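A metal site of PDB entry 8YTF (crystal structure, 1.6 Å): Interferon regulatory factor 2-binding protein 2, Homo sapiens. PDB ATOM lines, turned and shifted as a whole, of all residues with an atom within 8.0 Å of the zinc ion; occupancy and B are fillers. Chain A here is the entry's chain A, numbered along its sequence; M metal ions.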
ATOM      1  N   CYS A  10       9.363  12.820 -22.655  1.00  0.00           N
ATOM      2  CA  CYS A  10      10.574  12.911 -23.453  1.00  0.00           C
ATOM      3  C   CYS A  10      10.903  14.380 -23.734  1.00  0.00           C
ATOM      4  O   CYS A  10       9.997  15.198 -23.935  1.00  0.00           O
ATOM      5  CB  CYS A  10      10.324  12.156 -24.748  1.00  0.00           C
ATOM      6  SG  CYS A  10      10.632  10.369 -24.532  1.00  0.00           S
ATOM      7  N   CYS A  11      12.201  14.714 -23.736  1.00  0.00           N
ATOM      8  CA  CYS A  11      12.609  16.079 -24.086  1.00  0.00           C
ATOM      9  C   CYS A  11      12.206  16.404 -25.518  1.00  0.00           C
ATOM     10  O   CYS A  11      12.448  15.616 -26.441  1.00  0.00           O
ATOM     11  CB  CYS A  11      14.123  16.274 -23.910  1.00  0.00           C
ATOM     12  SG  CYS A  11      14.723  17.939 -24.361  1.00  0.00           S
ATOM     13  N   THR A  12      11.593  17.572 -25.694  1.00  0.00           N
ATOM     14  CA  THR A  12      11.139  18.012 -27.005  1.00  0.00           C
ATOM     15  C   THR A  12      12.284  18.086 -28.005  1.00  0.00           C
ATOM     16  O   THR A  12      12.084  17.806 -29.198  1.00  0.00           O
ATOM     17  CB  THR A  12      10.443  19.368 -26.840  1.00  0.00           C
ATOM     18  OG1 THR A  12       9.267  19.189 -26.053  1.00  0.00           O
ATOM     19  CG2 THR A  12      10.068  20.004 -28.182  1.00  0.00           C
ATOM     20  N   LEU A  13      13.489  18.448 -27.540  1.00  0.00           N
ATOM     21  CA  LEU A  13      14.589  18.726 -28.446  1.00  0.00           C
ATOM     22  C   LEU A  13      15.559  17.561 -28.604  1.00  0.00           C
ATOM     23  O   LEU A  13      16.010  17.313 -29.716  1.00  0.00           O
ATOM     24  CB  LEU A  13      15.344  19.983 -27.980  1.00  0.00           C
ATOM     25  CG  LEU A  13      14.449  21.213 -27.806  1.00  0.00           C
ATOM     26  CD1 LEU A  13      15.234  22.363 -27.207  1.00  0.00           C
ATOM     27  CD2 LEU A  13      13.808  21.675 -29.108  1.00  0.00           C
ATOM     28  N   CYS A  14      15.884  16.837 -27.537  1.00  0.00           N
ATOM     29  CA  CYS A  14      16.848  15.738 -27.645  1.00  0.00           C
ATOM     30  C   CYS A  14      16.245  14.359 -27.459  1.00  0.00           C
ATOM     31  O   CYS A  14      16.956  13.363 -27.660  1.00  0.00           O
ATOM     32  CB  CYS A  14      17.987  15.929 -26.623  1.00  0.00           C
ATOM     33  SG  CYS A  14      17.547  15.517 -24.946  1.00  0.00           S
ATOM     34  N   HIS A  15      14.966  14.268 -27.094  1.00  0.00           N
ATOM     35  CA  HIS A  15      14.178  13.033 -26.987  1.00  0.00           C
ATOM     36  C   HIS A  15      14.535  12.172 -25.787  1.00  0.00           C
ATOM     37  O   HIS A  15      14.017  11.058 -25.672  1.00  0.00           O
ATOM     38  CB  HIS A  15      14.305  12.193 -28.268  1.00  0.00           C
ATOM     39  CG  HIS A  15      14.187  12.995 -29.516  1.00  0.00           C
ATOM     40  ND1 HIS A  15      13.089  13.803 -29.773  1.00  0.00           N
ATOM     41  CD2 HIS A  15      15.033  13.171 -30.547  1.00  0.00           C
ATOM     42  CE1 HIS A  15      13.269  14.414 -30.924  1.00  0.00           C
ATOM     43  NE2 HIS A  15      14.440  14.054 -31.406  1.00  0.00           N
ATOM     44  N   GLU A  16      15.373  12.662 -24.888  1.00  0.00           N
ATOM     45  CA  GLU A  16      15.752  11.873 -23.729  1.00  0.00           C
ATOM     46  C   GLU A  16      14.602  11.792 -22.734  1.00  0.00           C
ATOM     47  O   GLU A  16      13.797  12.722 -22.605  1.00  0.00           O
ATOM     48  CB  GLU A  16      16.987  12.483 -23.070  1.00  0.00           C
ATOM     49  CG  GLU A  16      17.583  11.655 -21.962  1.00  0.00           C
ATOM     50  CD  GLU A  16      19.058  11.430 -22.200  1.00  0.00           C
ATOM     51  OE1 GLU A  16      19.716  12.351 -22.739  1.00  0.00           O
ATOM     52  OE2 GLU A  16      19.562  10.338 -21.874  1.00  0.00           O
ATOM     53  N   ARG A  17      14.520  10.669 -22.037  1.00  0.00           N
ATOM     54  CA  ARG A  17      13.500  10.513 -21.005  1.00  0.00           C
ATOM     55  C   ARG A  17      13.726  11.552 -19.914  1.00  0.00           C
ATOM     56  O   ARG A  17      14.859  11.769 -19.475  1.00  0.00           O
ATOM     57  CB  ARG A  17      13.555   9.110 -20.403  1.00  0.00           C
ATOM     58  CG  ARG A  17      13.264   7.958 -21.360  1.00  0.00           C
ATOM     59  CD  ARG A  17      11.821   7.542 -21.306  1.00  0.00           C
ATOM     60  NE  ARG A  17      11.427   7.074 -19.976  1.00  0.00           N
ATOM     61  CZ  ARG A  17      11.308   5.807 -19.606  1.00  0.00           C
ATOM     62  NH1 ARG A  17      11.634   4.801 -20.410  1.00  0.00           N
ATOM     63  NH2 ARG A  17      10.832   5.528 -18.395  1.00  0.00           N
ATOM     64  N   LEU A  18      12.655  12.198 -19.486  1.00  0.00           N
ATOM     65  CA  LEU A  18      12.762  13.135 -18.377  1.00  0.00           C
ATOM     66  C   LEU A  18      11.629  13.044 -17.367  1.00  0.00           C
ATOM     67  O   LEU A  18      11.594  13.854 -16.435  1.00  0.00           O
ATOM     68  CB  LEU A  18      12.894  14.578 -18.900  1.00  0.00           C
ATOM     69  CG  LEU A  18      12.026  15.078 -20.063  1.00  0.00           C
ATOM     70  CD1 LEU A  18      10.535  15.120 -19.699  1.00  0.00           C
ATOM     71  CD2 LEU A  18      12.507  16.466 -20.453  1.00  0.00           C
ATOM     72  N   LYS A  33       8.684  20.015 -23.153  1.00  0.00           N
ATOM     73  CA  LYS A  33       9.436  19.612 -21.975  1.00  0.00           C
ATOM     74  C   LYS A  33      10.912  19.599 -22.345  1.00  0.00           C
ATOM     75  O   LYS A  33      11.277  19.083 -23.400  1.00  0.00           O
ATOM     76  CB  LYS A  33       9.002  18.233 -21.489  1.00  0.00           C
ATOM     77  CG  LYS A  33       7.502  18.079 -21.275  1.00  0.00           C
ATOM     78  CD  LYS A  33       7.144  16.643 -20.839  1.00  0.00           C
ATOM     79  CE  LYS A  33       5.638  16.408 -20.911  1.00  0.00           C
ATOM     80  NZ  LYS A  33       4.860  17.201 -19.920  1.00  0.00           N
ATOM     81  N   PHE A  34      11.756  20.187 -21.506  1.00  0.00           N
ATOM     82  CA  PHE A  34      13.161  20.345 -21.867  1.00  0.00           C
ATOM     83  C   PHE A  34      14.062  19.935 -20.721  1.00  0.00           C
ATOM     84  O   PHE A  34      13.938  20.442 -19.609  1.00  0.00           O
ATOM     85  CB  PHE A  34      13.466  21.777 -22.306  1.00  0.00           C
ATOM     86  CG  PHE A  34      12.457  22.321 -23.265  1.00  0.00           C
ATOM     87  CD1 PHE A  34      12.573  22.063 -24.626  1.00  0.00           C
ATOM     88  CD2 PHE A  34      11.361  23.052 -22.811  1.00  0.00           C
ATOM     89  CE1 PHE A  34      11.622  22.544 -25.516  1.00  0.00           C
ATOM     90  CE2 PHE A  34      10.410  23.533 -23.701  1.00  0.00           C
ATOM     91  CZ  PHE A  34      10.551  23.276 -25.050  1.00  0.00           C
ATOM     92  N   CYS A  35      14.999  19.037 -21.013  1.00  0.00           N
ATOM     93  CA  CYS A  35      15.992  18.675 -20.017  1.00  0.00           C
ATOM     94  C   CYS A  35      16.893  19.867 -19.713  1.00  0.00           C
ATOM     95  O   CYS A  35      16.947  20.849 -20.463  1.00  0.00           O
ATOM     96  CB  CYS A  35      16.805  17.475 -20.497  1.00  0.00           C
ATOM     97  SG  CYS A  35      17.892  17.827 -21.909  1.00  0.00           S
ATOM     98  N   PHE A  36      17.618  19.782 -18.610  1.00  0.00           N
ATOM     99  CA  PHE A  36      18.493  20.898 -18.257  1.00  0.00           C
ATOM    100  C   PHE A  36      19.604  21.124 -19.276  1.00  0.00           C
ATOM    101  O   PHE A  36      19.851  22.300 -19.605  1.00  0.00           O
ATOM    102  CB  PHE A  36      19.098  20.700 -16.855  1.00  0.00           C
ATOM    103  CG  PHE A  36      18.200  21.128 -15.724  1.00  0.00           C
ATOM    104  CD1 PHE A  36      16.851  21.374 -15.915  1.00  0.00           C
ATOM    105  CD2 PHE A  36      18.725  21.299 -14.455  1.00  0.00           C
ATOM    106  CE1 PHE A  36      16.041  21.772 -14.864  1.00  0.00           C
ATOM    107  CE2 PHE A  36      17.931  21.685 -13.403  1.00  0.00           C
ATOM    108  CZ  PHE A  36      16.590  21.925 -13.593  1.00  0.00           C
ATOM    109  N   PRO A  37      20.289  20.109 -19.828  1.00  0.00           N
ATOM    110  CA  PRO A  37      21.278  20.386 -20.879  1.00  0.00           C
ATOM    111  C   PRO A  37      20.732  21.152 -22.064  1.00  0.00           C
ATOM    112  O   PRO A  37      21.337  22.132 -22.519  1.00  0.00           O
ATOM    113  CB  PRO A  37      21.786  18.985 -21.267  1.00  0.00           C
ATOM    114  CG  PRO A  37      21.629  18.201 -20.040  1.00  0.00           C
ATOM    115  CD  PRO A  37      20.371  18.703 -19.381  1.00  0.00           C
ATOM    116  N   CYS A  38      19.563  20.747 -22.580  1.00  0.00           N
ATOM    117  CA  CYS A  38      18.998  21.480 -23.704  1.00  0.00           C
ATOM    118  C   CYS A  38      18.586  22.879 -23.287  1.00  0.00           C
ATOM    119  O   CYS A  38      18.714  23.836 -24.072  1.00  0.00           O
ATOM    120  CB  CYS A  38      17.807  20.712 -24.270  1.00  0.00           C
ATOM    121  SG  CYS A  38      18.261  19.215 -25.185  1.00  0.00           S
ATOM    122  N   SER A  39      18.062  23.030 -22.074  1.00  0.00           N
ATOM    123  CA  SER A  39      17.674  24.339 -21.578  1.00  0.00           C
ATOM    124  C   SER A  39      18.880  25.263 -21.445  1.00  0.00           C
ATOM    125  O   SER A  39      18.777  26.471 -21.704  1.00  0.00           O
ATOM    126  CB  SER A  39      16.961  24.218 -20.227  1.00  0.00           C
ATOM    127  OG  SER A  39      15.739  23.503 -20.359  1.00  0.00           O
HETATM  128 ZN    ZN M   1      17.035  17.633 -24.117  1.00  0.00          ZN
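The backbone NH (N) of Glu 16 lies close to the side-chain sulfur (SG) of Cys 14 (3.6 Å). The side-chain hydroxyl (OG) of Ser 39 is in hydrogen-bond range of the backbone carbonyl oxygen (O) of Cys 35, 2.9 Å away. The side-chain sulfur (SG) of Cys 11 lies close to the backbone carbonyl oxygen (O) of Lys 33 (3.8 Å). O of Glu 16 sits at hydrogen-bond distance from N of Cys 11, at 2.8 Å. The side-chain sulfur (SG) of Cys 11 lies close to the backbone NH (N) of Leu 13 (3.4 Å).
The zinc ion is bound by the side-chain sulfur of Cys 38 (2.3 Å), the side-chain sulfur of Cys 14 (2.3 Å), the side-chain sulfur of Cys 11 (2.3 Å) and the side-chain sulfur of Cys 35 (2.4 Å).
Of the 16 residues printed, 4 come within 4 Å of the zinc ion. Along chain A the residues within 4 Å of the zinc ion span positions 11 to 38.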
